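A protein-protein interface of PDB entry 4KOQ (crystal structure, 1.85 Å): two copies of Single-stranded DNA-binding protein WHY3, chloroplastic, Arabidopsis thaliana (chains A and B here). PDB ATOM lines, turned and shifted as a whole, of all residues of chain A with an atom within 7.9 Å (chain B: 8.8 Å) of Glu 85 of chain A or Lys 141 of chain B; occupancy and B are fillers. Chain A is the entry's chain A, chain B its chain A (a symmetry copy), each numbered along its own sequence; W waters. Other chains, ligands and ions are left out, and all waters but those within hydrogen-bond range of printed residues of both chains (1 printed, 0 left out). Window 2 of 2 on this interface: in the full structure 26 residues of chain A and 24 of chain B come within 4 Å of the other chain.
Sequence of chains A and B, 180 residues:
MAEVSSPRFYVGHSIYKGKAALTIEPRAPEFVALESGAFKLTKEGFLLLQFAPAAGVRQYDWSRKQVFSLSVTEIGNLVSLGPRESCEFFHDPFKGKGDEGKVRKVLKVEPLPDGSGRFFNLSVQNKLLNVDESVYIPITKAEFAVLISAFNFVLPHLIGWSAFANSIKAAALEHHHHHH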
ATOM      1  N   THR A  73     -23.608  27.071  14.038  1.00  0.00           N
ATOM      2  CA  THR A  73     -22.936  26.404  12.908  1.00  0.00           C
ATOM      3  C   THR A  73     -23.133  24.901  12.977  1.00  0.00           C
ATOM      4  O   THR A  73     -23.375  24.266  11.982  1.00  0.00           O
ATOM      5  CB  THR A  73     -21.422  26.728  12.881  1.00  0.00           C
ATOM      6  OG1 THR A  73     -21.261  28.141  12.723  1.00  0.00           O
ATOM      7  CG2 THR A  73     -20.721  26.021  11.729  1.00  0.00           C
ATOM      8  N   GLY A  76     -26.340  24.060  11.792  1.00  0.00           N
ATOM      9  CA  GLY A  76     -26.280  24.038  10.354  1.00  0.00           C
ATOM     10  C   GLY A  76     -25.747  22.737   9.766  1.00  0.00           C
ATOM     11  O   GLY A  76     -26.241  22.252   8.737  1.00  0.00           O
ATOM     12  N   ASN A  77     -24.759  22.150  10.424  1.00  0.00           N
ATOM     13  CA  ASN A  77     -24.278  20.866   9.976  1.00  0.00           C
ATOM     14  C   ASN A  77     -25.364  19.807  10.001  1.00  0.00           C
ATOM     15  O   ASN A  77     -25.503  19.038   9.063  1.00  0.00           O
ATOM     16  CB  ASN A  77     -23.159  20.409  10.870  1.00  0.00           C
ATOM     17  CG  ASN A  77     -22.205  19.505  10.160  1.00  0.00           C
ATOM     18  OD1 ASN A  77     -22.583  18.719   9.273  1.00  0.00           O
ATOM     19  ND2 ASN A  77     -20.951  19.659  10.474  1.00  0.00           N
ATOM     20  N   LEU A  78     -26.109  19.773  11.094  1.00  0.00           N
ATOM     21  CA  LEU A  78     -27.155  18.763  11.277  1.00  0.00           C
ATOM     22  C   LEU A  78     -28.252  18.921  10.267  1.00  0.00           C
ATOM     23  O   LEU A  78     -28.790  17.934   9.787  1.00  0.00           O
ATOM     24  CB  LEU A  78     -27.733  18.825  12.691  1.00  0.00           C
ATOM     25  CG  LEU A  78     -26.743  18.371  13.758  1.00  0.00           C
ATOM     26  CD1 LEU A  78     -27.367  18.455  15.116  1.00  0.00           C
ATOM     27  CD2 LEU A  78     -26.358  16.950  13.456  1.00  0.00           C
ATOM     28  N   VAL A  79     -28.648  20.153   9.950  1.00  0.00           N
ATOM     29  CA  VAL A  79     -29.754  20.318   9.018  1.00  0.00           C
ATOM     30  C   VAL A  79     -29.318  20.105   7.559  1.00  0.00           C
ATOM     31  O   VAL A  79     -30.154  20.074   6.672  1.00  0.00           O
ATOM     32  CB  VAL A  79     -30.490  21.725   9.095  1.00  0.00           C
ATOM     33  CG1 VAL A  79     -31.149  21.924  10.439  1.00  0.00           C
ATOM     34  CG2 VAL A  79     -29.562  22.841   8.753  1.00  0.00           C
ATOM     35  N   SER A  80     -28.035  19.940   7.309  1.00  0.00           N
ATOM     36  CA  SER A  80     -27.572  19.710   5.939  1.00  0.00           C
ATOM     37  C   SER A  80     -26.941  18.348   5.739  1.00  0.00           C
ATOM     38  O   SER A  80     -26.316  18.123   4.720  1.00  0.00           O
ATOM     39  CB  SER A  80     -26.568  20.781   5.499  1.00  0.00           C
ATOM     40  OG  SER A  80     -25.469  20.876   6.345  1.00  0.00           O
ATOM     41  N   LEU A  81     -27.098  17.431   6.691  1.00  0.00           N
ATOM     42  CA  LEU A  81     -26.466  16.129   6.529  1.00  0.00           C
ATOM     43  C   LEU A  81     -27.055  15.339   5.365  1.00  0.00           C
ATOM     44  O   LEU A  81     -28.250  15.194   5.276  1.00  0.00           O
ATOM     45  CB  LEU A  81     -26.655  15.306   7.793  1.00  0.00           C
ATOM     46  CG  LEU A  81     -25.809  15.674   8.984  1.00  0.00           C
ATOM     47  CD1 LEU A  81     -26.137  14.733  10.160  1.00  0.00           C
ATOM     48  CD2 LEU A  81     -24.296  15.559   8.656  1.00  0.00           C
ATOM     49  N   GLY A  82     -26.199  14.789   4.516  1.00  0.00           N
ATOM     50  CA  GLY A  82     -26.639  13.815   3.537  1.00  0.00           C
ATOM     51  C   GLY A  82     -27.059  12.517   4.220  1.00  0.00           C
ATOM     52  O   GLY A  82     -26.717  12.291   5.371  1.00  0.00           O
ATOM     53  N   PRO A  83     -27.788  11.653   3.509  1.00  0.00           N
ATOM     54  CA  PRO A  83     -28.291  10.381   4.052  1.00  0.00           C
ATOM     55  C   PRO A  83     -27.212   9.413   4.540  1.00  0.00           C
ATOM     56  O   PRO A  83     -27.513   8.593   5.400  1.00  0.00           O
ATOM     57  CB  PRO A  83     -29.034   9.754   2.863  1.00  0.00           C
ATOM     58  CG  PRO A  83     -29.198  10.840   1.875  1.00  0.00           C
ATOM     59  CD  PRO A  83     -28.077  11.787   2.070  1.00  0.00           C
ATOM     60  N   ARG A  84     -25.980   9.506   4.057  1.00  0.00           N
ATOM     61  CA  ARG A  84     -24.936   8.586   4.517  1.00  0.00           C
ATOM     62  C   ARG A  84     -23.788   9.320   5.188  1.00  0.00           C
ATOM     63  O   ARG A  84     -22.744   8.746   5.485  1.00  0.00           O
ATOM     64  CB  ARG A  84     -24.473   7.727   3.346  1.00  0.00           C
ATOM     65  CG  ARG A  84     -25.678   7.240   2.524  1.00  0.00           C
ATOM     66  CD  ARG A  84     -25.407   5.956   1.769  1.00  0.00           C
ATOM     67  NE  ARG A  84     -24.216   6.031   0.926  1.00  0.00           N
ATOM     68  CZ  ARG A  84     -23.134   5.264   1.060  1.00  0.00           C
ATOM     69  NH1 ARG A  84     -22.114   5.421   0.226  1.00  0.00           N
ATOM     70  NH2 ARG A  84     -23.053   4.340   2.012  1.00  0.00           N
ATOM     71  N   GLU A  85     -24.031  10.595   5.478  1.00  0.00           N
ATOM     72  CA  GLU A  85     -23.028  11.449   6.050  1.00  0.00           C
ATOM     73  C   GLU A  85     -23.105  11.451   7.582  1.00  0.00           C
ATOM     74  O   GLU A  85     -24.198  11.387   8.150  1.00  0.00           O
ATOM     75  CB  GLU A  85     -23.225  12.878   5.518  1.00  0.00           C
ATOM     76  CG  GLU A  85     -22.090  13.822   5.866  1.00  0.00           C
ATOM     77  CD  GLU A  85     -22.261  15.222   5.253  1.00  0.00           C
ATOM     78  OE1 GLU A  85     -23.323  15.527   4.663  1.00  0.00           O
ATOM     79  OE2 GLU A  85     -21.315  16.016   5.377  1.00  0.00           O
ATOM     80  N   SER A  86     -21.947  11.546   8.221  1.00  0.00           N
ATOM     81  CA  SER A  86     -21.859  11.714   9.660  1.00  0.00           C
ATOM     82  C   SER A  86     -21.240  13.044   9.968  1.00  0.00           C
ATOM     83  O   SER A  86     -20.595  13.647   9.104  1.00  0.00           O
ATOM     84  CB  SER A  86     -21.057  10.563  10.288  1.00  0.00           C
ATOM     85  OG  SER A  86     -19.648  10.768  10.159  1.00  0.00           O
ATOM     86  N   CYS A  87     -21.486  13.554  11.166  1.00  0.00           N
ATOM     87  CA  CYS A  87     -20.759  14.704  11.637  1.00  0.00           C
ATOM     88  C   CYS A  87     -20.297  14.466  13.078  1.00  0.00           C
ATOM     89  O   CYS A  87     -20.874  13.661  13.809  1.00  0.00           O
ATOM     90  CB  CYS A  87     -21.607  15.986  11.519  1.00  0.00           C
ATOM     91  SG  CYS A  87     -23.089  15.970  12.458  1.00  0.00           S
ATOM     92  N   LYS A 108     -21.147  12.867  18.237  1.00  0.00           N
ATOM     93  CA  LYS A 108     -21.150  12.314  16.895  1.00  0.00           C
ATOM     94  C   LYS A 108     -22.563  11.939  16.477  1.00  0.00           C
ATOM     95  O   LYS A 108     -23.337  11.397  17.273  1.00  0.00           O
ATOM     96  CB  LYS A 108     -20.251  11.072  16.786  1.00  0.00           C
ATOM     97  CG  LYS A 108     -20.039  10.637  15.375  1.00  0.00           C
ATOM     98  CD  LYS A 108     -18.993   9.554  15.198  1.00  0.00           C
ATOM     99  CE  LYS A 108     -18.659   9.403  13.728  1.00  0.00           C
ATOM    100  NZ  LYS A 108     -18.113   8.055  13.447  1.00  0.00           N
ATOM    101  N   VAL A 109     -22.896  12.251  15.229  1.00  0.00           N
ATOM    102  CA  VAL A 109     -24.163  11.903  14.642  1.00  0.00           C
ATOM    103  C   VAL A 109     -23.972  11.103  13.363  1.00  0.00           C
ATOM    104  O   VAL A 109     -23.341  11.579  12.404  1.00  0.00           O
ATOM    105  CB  VAL A 109     -25.058  13.153  14.351  1.00  0.00           C
ATOM    106  CG1 VAL A 109     -26.349  12.696  13.745  1.00  0.00           C
ATOM    107  CG2 VAL A 109     -25.345  13.912  15.623  1.00  0.00           C
ATOM    108  N   GLU A 110     -24.531   9.898  13.353  1.00  0.00           N
ATOM    109  CA  GLU A 110     -24.285   8.922  12.312  1.00  0.00           C
ATOM    110  C   GLU A 110     -25.576   8.395  11.741  1.00  0.00           C
ATOM    111  O   GLU A 110     -26.583   8.322  12.427  1.00  0.00           O
ATOM    112  CB  GLU A 110     -23.543   7.719  12.896  1.00  0.00           C
ATOM    113  CG  GLU A 110     -22.110   7.933  13.225  1.00  0.00           C
ATOM    114  CD  GLU A 110     -21.530   6.734  13.971  1.00  0.00           C
ATOM    115  OE1 GLU A 110     -22.236   6.189  14.849  1.00  0.00           O
ATOM    116  OE2 GLU A 110     -20.381   6.340  13.684  1.00  0.00           O
ATOM    117  N   PRO A 111     -25.545   7.982  10.472  1.00  0.00           N
ATOM    118  CA  PRO A 111     -26.712   7.369   9.856  1.00  0.00           C
ATOM    119  C   PRO A 111     -26.885   5.977  10.427  1.00  0.00           C
ATOM    120  O   PRO A 111     -25.879   5.362  10.775  1.00  0.00           O
ATOM    121  CB  PRO A 111     -26.330   7.314   8.362  1.00  0.00           C
ATOM    122  CG  PRO A 111     -24.850   7.330   8.344  1.00  0.00           C
ATOM    123  CD  PRO A 111     -24.403   8.096   9.539  1.00  0.00           C
ATOM    124  N   LEU A 112     -28.122   5.521  10.604  1.00  0.00           N
ATOM    125  CA  LEU A 112     -28.340   4.125  10.978  1.00  0.00           C
ATOM    126  C   LEU A 112     -28.239   3.292   9.702  1.00  0.00           C
ATOM    127  O   LEU A 112     -28.728   3.708   8.649  1.00  0.00           O
ATOM    128  CB  LEU A 112     -29.686   3.926  11.679  1.00  0.00           C
ATOM    129  CG  LEU A 112     -29.768   4.543  13.074  1.00  0.00           C
ATOM    130  CD1 LEU A 112     -31.205   4.530  13.564  1.00  0.00           C
ATOM    131  CD2 LEU A 112     -28.871   3.837  14.052  1.00  0.00           C
ATOM    132  N   GLY A 117     -32.839   6.152  10.251  1.00  0.00           N
ATOM    133  CA  GLY A 117     -32.681   7.260  11.191  1.00  0.00           C
ATOM    134  C   GLY A 117     -31.249   7.559  11.528  1.00  0.00           C
ATOM    135  O   GLY A 117     -30.364   7.351  10.691  1.00  0.00           O
ATOM    136  N   ARG A 118     -31.025   8.086  12.732  1.00  0.00           N
ATOM    137  CA  ARG A 118     -29.703   8.590  13.132  1.00  0.00           C
ATOM    138  C   ARG A 118     -29.299   8.076  14.512  1.00  0.00           C
ATOM    139  O   ARG A 118     -30.133   7.828  15.379  1.00  0.00           O
ATOM    140  CB  ARG A 118     -29.676  10.121  13.138  1.00  0.00           C
ATOM    141  CG  ARG A 118     -29.992  10.780  11.794  1.00  0.00           C
ATOM    142  CD  ARG A 118     -28.776  10.895  10.944  1.00  0.00           C
ATOM    143  NE  ARG A 118     -29.079  11.412   9.628  1.00  0.00           N
ATOM    144  CZ  ARG A 118     -28.191  11.548   8.658  1.00  0.00           C
ATOM    145  NH1 ARG A 118     -26.940  11.175   8.839  1.00  0.00           N
ATOM    146  NH2 ARG A 118     -28.578  12.016   7.487  1.00  0.00           N
ATOM    147  N   LYS B  17     -12.789  33.868   9.283  1.00  0.00           N
ATOM    148  CA  LYS B  17     -11.879  32.889   8.774  1.00  0.00           C
ATOM    149  C   LYS B  17     -10.445  33.401   8.847  1.00  0.00           C
ATOM    150  O   LYS B  17     -10.182  34.518   9.308  1.00  0.00           O
ATOM    151  CB  LYS B  17     -12.260  32.488   7.334  1.00  0.00           C
ATOM    152  CG  LYS B  17     -13.577  31.696   7.239  1.00  0.00           C
ATOM    153  CD  LYS B  17     -13.497  30.326   7.945  1.00  0.00           C
ATOM    154  CE  LYS B  17     -14.877  29.740   8.163  1.00  0.00           C
ATOM    155  NZ  LYS B  17     -15.342  29.061   6.945  1.00  0.00           N
ATOM    156  N   PRO B  83     -25.641  22.185  -6.437  1.00  0.00           N
ATOM    157  CA  PRO B  83     -24.340  21.839  -5.843  1.00  0.00           C
ATOM    158  C   PRO B  83     -23.122  22.206  -6.691  1.00  0.00           C
ATOM    159  O   PRO B  83     -22.054  22.398  -6.122  1.00  0.00           O
ATOM    160  CB  PRO B  83     -24.412  20.312  -5.694  1.00  0.00           C
ATOM    161  CG  PRO B  83     -25.835  19.958  -5.873  1.00  0.00           C
ATOM    162  CD  PRO B  83     -26.437  20.986  -6.751  1.00  0.00           C
ATOM    163  N   LEU B 112     -17.102  24.903  -3.652  1.00  0.00           N
ATOM    164  CA  LEU B 112     -15.728  24.475  -3.394  1.00  0.00           C
ATOM    165  C   LEU B 112     -15.544  23.115  -4.063  1.00  0.00           C
ATOM    166  O   LEU B 112     -16.446  22.274  -4.019  1.00  0.00           O
ATOM    167  CB  LEU B 112     -15.421  24.417  -1.897  1.00  0.00           C
ATOM    168  CG  LEU B 112     -15.359  25.781  -1.211  1.00  0.00           C
ATOM    169  CD1 LEU B 112     -15.322  25.604   0.296  1.00  0.00           C
ATOM    170  CD2 LEU B 112     -14.179  26.588  -1.678  1.00  0.00           C
ATOM    171  N   ASP B 114     -14.330  20.332  -3.820  1.00  0.00           N
ATOM    172  CA  ASP B 114     -14.486  19.024  -3.199  1.00  0.00           C
ATOM    173  C   ASP B 114     -15.848  18.831  -2.539  1.00  0.00           C
ATOM    174  O   ASP B 114     -16.056  17.833  -1.848  1.00  0.00           O
ATOM    175  CB  ASP B 114     -13.370  18.789  -2.181  1.00  0.00           C
ATOM    176  CG  ASP B 114     -13.217  19.940  -1.219  1.00  0.00           C
ATOM    177  OD1 ASP B 114     -14.149  20.775  -1.144  1.00  0.00           O
ATOM    178  OD2 ASP B 114     -12.170  20.009  -0.540  1.00  0.00           O
ATOM    179  N   GLY B 115     -16.775  19.768  -2.749  1.00  0.00           N
ATOM    180  CA  GLY B 115     -18.143  19.623  -2.237  1.00  0.00           C
ATOM    181  C   GLY B 115     -18.334  20.098  -0.799  1.00  0.00           C
ATOM    182  O   GLY B 115     -19.400  19.922  -0.194  1.00  0.00           O
ATOM    183  N   SER B 116     -17.293  20.708  -0.252  1.00  0.00           N
ATOM    184  CA  SER B 116     -17.243  21.016   1.164  1.00  0.00           C
ATOM    185  C   SER B 116     -17.798  22.407   1.489  1.00  0.00           C
ATOM    186  O   SER B 116     -17.637  22.884   2.606  1.00  0.00           O
ATOM    187  CB  SER B 116     -15.796  20.970   1.618  1.00  0.00           C
ATOM    188  OG  SER B 116     -15.040  21.855   0.817  1.00  0.00           O
ATOM    189  N   GLY B 117     -18.448  23.067   0.542  1.00  0.00           N
ATOM    190  CA  GLY B 117     -18.991  24.387   0.856  1.00  0.00           C
ATOM    191  C   GLY B 117     -18.915  25.353  -0.291  1.00  0.00           C
ATOM    192  O   GLY B 117     -18.984  24.935  -1.452  1.00  0.00           O
ATOM    193  N   ARG B 118     -18.817  26.643   0.032  1.00  0.00           N
ATOM    194  CA  ARG B 118     -18.910  27.709  -0.976  1.00  0.00           C
ATOM    195  C   ARG B 118     -17.787  28.733  -0.815  1.00  0.00           C
ATOM    196  O   ARG B 118     -17.294  28.985   0.280  1.00  0.00           O
ATOM    197  CB  ARG B 118     -20.260  28.428  -0.895  1.00  0.00           C
ATOM    198  CG  ARG B 118     -21.483  27.534  -1.111  1.00  0.00           C
ATOM    199  CD  ARG B 118     -21.800  27.384  -2.558  1.00  0.00           C
ATOM    200  NE  ARG B 118     -22.883  26.453  -2.783  1.00  0.00           N
ATOM    201  CZ  ARG B 118     -23.316  26.089  -3.979  1.00  0.00           C
ATOM    202  NH1 ARG B 118     -22.738  26.551  -5.069  1.00  0.00           N
ATOM    203  NH2 ARG B 118     -24.302  25.218  -4.072  1.00  0.00           N
ATOM    204  N   PHE B 119     -17.422  29.357  -1.926  1.00  0.00           N
ATOM    205  CA  PHE B 119     -16.387  30.375  -1.933  1.00  0.00           C
ATOM    206  C   PHE B 119     -17.071  31.669  -2.292  1.00  0.00           C
ATOM    207  O   PHE B 119     -17.618  31.764  -3.370  1.00  0.00           O
ATOM    208  CB  PHE B 119     -15.337  29.965  -2.981  1.00  0.00           C
ATOM    209  CG  PHE B 119     -13.958  30.534  -2.763  1.00  0.00           C
ATOM    210  CD1 PHE B 119     -13.409  30.664  -1.481  1.00  0.00           C
ATOM    211  CD2 PHE B 119     -13.174  30.882  -3.849  1.00  0.00           C
ATOM    212  CE1 PHE B 119     -12.112  31.169  -1.291  1.00  0.00           C
ATOM    213  CE2 PHE B 119     -11.880  31.375  -3.665  1.00  0.00           C
ATOM    214  CZ  PHE B 119     -11.348  31.511  -2.375  1.00  0.00           C
ATOM    215  N   PRO B 138     -13.932  31.510   2.321  1.00  0.00           N
ATOM    216  CA  PRO B 138     -14.564  30.196   2.204  1.00  0.00           C
ATOM    217  C   PRO B 138     -15.623  29.976   3.286  1.00  0.00           C
ATOM    218  O   PRO B 138     -15.450  30.387   4.442  1.00  0.00           O
ATOM    219  CB  PRO B 138     -13.399  29.232   2.432  1.00  0.00           C
ATOM    220  CG  PRO B 138     -12.488  29.981   3.318  1.00  0.00           C
ATOM    221  CD  PRO B 138     -12.634  31.441   2.999  1.00  0.00           C
ATOM    222  N   ILE B 139     -16.711  29.348   2.880  1.00  0.00           N
ATOM    223  CA  ILE B 139     -17.890  29.133   3.727  1.00  0.00           C
ATOM    224  C   ILE B 139     -18.114  27.622   3.689  1.00  0.00           C
ATOM    225  O   ILE B 139     -18.282  27.062   2.603  1.00  0.00           O
ATOM    226  CB  ILE B 139     -19.114  29.895   3.088  1.00  0.00           C
ATOM    227  CG1 ILE B 139     -18.811  31.404   2.905  1.00  0.00           C
ATOM    228  CG2 ILE B 139     -20.393  29.769   3.879  1.00  0.00           C
ATOM    229  CD1 ILE B 139     -18.508  32.113   4.216  1.00  0.00           C
ATOM    230  N   THR B 140     -18.119  26.963   4.836  1.00  0.00           N
ATOM    231  CA  THR B 140     -18.385  25.516   4.874  1.00  0.00           C
ATOM    232  C   THR B 140     -19.807  25.211   4.510  1.00  0.00           C
ATOM    233  O   THR B 140     -20.684  26.079   4.584  1.00  0.00           O
ATOM    234  CB  THR B 140     -18.104  24.877   6.257  1.00  0.00           C
ATOM    235  OG1 THR B 140     -19.023  25.384   7.236  1.00  0.00           O
ATOM    236  CG2 THR B 140     -16.637  25.124   6.720  1.00  0.00           C
ATOM    237  N   LYS B 141     -20.085  23.942   4.180  1.00  0.00           N
ATOM    238  CA  LYS B 141     -21.458  23.510   3.904  1.00  0.00           C
ATOM    239  C   LYS B 141     -22.383  23.837   5.098  1.00  0.00           C
ATOM    240  O   LYS B 141     -23.527  24.259   4.890  1.00  0.00           O
ATOM    241  CB  LYS B 141     -21.482  21.993   3.589  1.00  0.00           C
ATOM    242  CG  LYS B 141     -22.840  21.403   3.324  1.00  0.00           C
ATOM    243  CD  LYS B 141     -22.691  19.904   3.051  1.00  0.00           C
ATOM    244  CE  LYS B 141     -24.010  19.211   2.820  1.00  0.00           C
ATOM    245  NZ  LYS B 141     -23.820  17.717   2.904  1.00  0.00           N
ATOM    246  N   ALA B 142     -21.889  23.633   6.319  1.00  0.00           N
ATOM    247  CA  ALA B 142     -22.662  23.907   7.539  1.00  0.00           C
ATOM    248  C   ALA B 142     -22.950  25.388   7.709  1.00  0.00           C
ATOM    249  O   ALA B 142     -24.055  25.791   8.044  1.00  0.00           O
ATOM    250  CB  ALA B 142     -21.920  23.405   8.731  1.00  0.00           C
ATOM    251  N   GLU B 143     -21.953  26.220   7.440  1.00  0.00           N
ATOM    252  CA  GLU B 143     -22.145  27.672   7.522  1.00  0.00           C
ATOM    253  C   GLU B 143     -23.096  28.145   6.431  1.00  0.00           C
ATOM    254  O   GLU B 143     -23.951  29.009   6.654  1.00  0.00           O
ATOM    255  CB  GLU B 143     -20.782  28.407   7.421  1.00  0.00           C
ATOM    256  CG  GLU B 143     -19.913  28.250   8.642  1.00  0.00           C
ATOM    257  CD  GLU B 143     -18.421  28.506   8.400  1.00  0.00           C
ATOM    258  OE1 GLU B 143     -17.948  28.508   7.237  1.00  0.00           O
ATOM    259  OE2 GLU B 143     -17.726  28.719   9.404  1.00  0.00           O
ATOM    260  N   PHE B 144     -22.983  27.575   5.248  1.00  0.00           N
ATOM    261  CA  PHE B 144     -23.871  27.952   4.164  1.00  0.00           C
ATOM    262  C   PHE B 144     -25.302  27.528   4.495  1.00  0.00           C
ATOM    263  O   PHE B 144     -26.265  28.225   4.162  1.00  0.00           O
ATOM    264  CB  PHE B 144     -23.383  27.400   2.813  1.00  0.00           C
ATOM    265  CG  PHE B 144     -24.076  28.009   1.635  1.00  0.00           C
ATOM    266  CD1 PHE B 144     -23.821  29.328   1.287  1.00  0.00           C
ATOM    267  CD2 PHE B 144     -24.949  27.282   0.871  1.00  0.00           C
ATOM    268  CE1 PHE B 144     -24.498  29.925   0.194  1.00  0.00           C
ATOM    269  CE2 PHE B 144     -25.611  27.867  -0.231  1.00  0.00           C
ATOM    270  CZ  PHE B 144     -25.366  29.187  -0.552  1.00  0.00           C
ATOM    271  N   ALA B 145     -25.473  26.385   5.162  1.00  0.00           N
ATOM    272  CA  ALA B 145     -26.815  25.946   5.561  1.00  0.00           C
ATOM    273  C   ALA B 145     -27.503  26.917   6.543  1.00  0.00           C
ATOM    274  O   ALA B 145     -28.739  27.105   6.488  1.00  0.00           O
ATOM    275  CB  ALA B 145     -26.773  24.496   6.198  1.00  0.00           C
ATOM    276  N   VAL B 146     -26.710  27.495   7.431  1.00  0.00           N
ATOM    277  CA  VAL B 146     -27.182  28.513   8.356  1.00  0.00           C
ATOM    278  C   VAL B 146     -27.685  29.690   7.514  1.00  0.00           C
ATOM    279  O   VAL B 146     -28.771  30.221   7.761  1.00  0.00           O
ATOM    280  CB  VAL B 146     -26.090  28.990   9.286  1.00  0.00           C
ATOM    281  CG1 VAL B 146     -26.549  30.194  10.139  1.00  0.00           C
ATOM    282  CG2 VAL B 146     -25.666  27.860  10.225  1.00  0.00           C
ATOM    283  N   LEU B 147     -26.881  30.122   6.546  1.00  0.00           N
ATOM    284  CA  LEU B 147     -27.344  31.209   5.632  1.00  0.00           C
ATOM    285  C   LEU B 147     -28.619  30.885   4.888  1.00  0.00           C
ATOM    286  O   LEU B 147     -29.546  31.715   4.826  1.00  0.00           O
ATOM    287  CB  LEU B 147     -26.242  31.609   4.635  1.00  0.00           C
ATOM    288  CG  LEU B 147     -24.933  32.081   5.232  1.00  0.00           C
ATOM    289  CD1 LEU B 147     -23.916  32.536   4.162  1.00  0.00           C
ATOM    290  CD2 LEU B 147     -25.154  33.187   6.256  1.00  0.00           C
ATOM    291  N   ILE B 148     -28.704  29.700   4.305  1.00  0.00           N
ATOM    292  CA  ILE B 148     -29.947  29.307   3.652  1.00  0.00           C
ATOM    293  C   ILE B 148     -31.153  29.388   4.586  1.00  0.00           C
ATOM    294  O   ILE B 148     -32.219  29.911   4.203  1.00  0.00           O
ATOM    295  CB  ILE B 148     -29.862  27.899   3.013  1.00  0.00           C
ATOM    296  CG1 ILE B 148     -28.809  27.850   1.912  1.00  0.00           C
ATOM    297  CG2 ILE B 148     -31.211  27.503   2.429  1.00  0.00           C
ATOM    298  CD1 ILE B 148     -28.535  26.421   1.451  1.00  0.00           C
HETATM  299  O   HOH W   1     -18.608  29.574  11.628  1.00  0.00           O
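Of the printed residues of chain B, Asn 77 of chain A touches Ala 142.
Glu 85 of chain A touches one residue of chain B.
No residue of chain B comes within 4 Å of Ser 86 of chain A.
Lys 141 of chain B touches just these residues of chain A: Ser 80 and Glu 85.
Of the printed residues of chain A, Ala 142 of chain B touches Thr 73, Gly 76 and Asn 77.
Printed residues of chain A within 4 Å of Glu 143 of chain B: Thr 73.
Printed residues of chain A within 4 Å of Ala 145 of chain B: Gly 76 (3.4 Å) and Ser 80 (3.8 Å).
The nearest residue of chain B that does not touch Glu 85 of chain A is Gly 115 of chain B (7.1 Å).
Among the printed residues, Asp or Glu carboxylates within 4 Å of a Lys or Arg side-chain nitrogen of the other chain: Glu 85 of chain A with Lys 141 of chain B (2.9 Å).
O of Thr 73 of chain A touches CB of Ala 142 of chain B, at 3.7 Å.
CG of Glu 143 of chain B touches CG2 of Thr 73 of chain A, 3.9 Å away.
Gly 76 of chain A touches Ala 142 of chain B (CA to O, 3.7 Å).
Gly 76 of chain A touches Ala 145 of chain B.
Gly 76 of chain A touches Val 146 of chain B (CA to CG2, 3.9 Å).
Asn 77 of chain A touches Ala 142 of chain B.
Ser 80 of chain A touches Ala 145 of chain B.
The backbone carbonyl oxygen (O) of Gly 76 of chain A sits at hydrogen-bond distance from the side-chain hydroxyl (OG) of Ser 80 of chain A (2.9 Å).
The backbone NH (N) of Lys 141 of chain B sits at hydrogen-bond distance from the backbone carbonyl oxygen (O) of Ser 116 of chain B (3.1 Å).
The backbone NH (N) of Gly 82 of chain A is in hydrogen-bond range of the side-chain carboxylate (OE1) of Glu 85 of chain A, 3.0 Å away.
The side-chain hydroxyl (OG1) of Thr 140 of chain B sits close to the backbone NH (N) of Ala 142 of chain B (3.5 Å).
O of Glu 85 of chain A lies within hydrogen-bond range of NH1 of Arg 118 of chain A (2.8 Å).
O of Asn 77 of chain A sits at hydrogen-bond distance from OG of Ser 80 of chain A (3.3 Å).
Water W1 lies within hydrogen-bond range of the side-chain carboxylate of Glu 143 of chain B (2.5 Å) and the side-chain hydroxyl of Thr 73 of chain A (3.2 Å).
Positions printed for both chains: 83, 112, 117 and 118.
Of the 9 pairs that touch across the chains among the printed residues, none has its exchanged pair printed and touching as well.
The side-chain carboxylate of Glu 85 of chain A lies within salt-bridge range of the side-chain amino group of Lys 141 of chain B (2.9 Å).
O of Ser 80 of chain A sits at hydrogen-bond distance from NZ of Lys 141 of chain B, at 3.1 Å.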
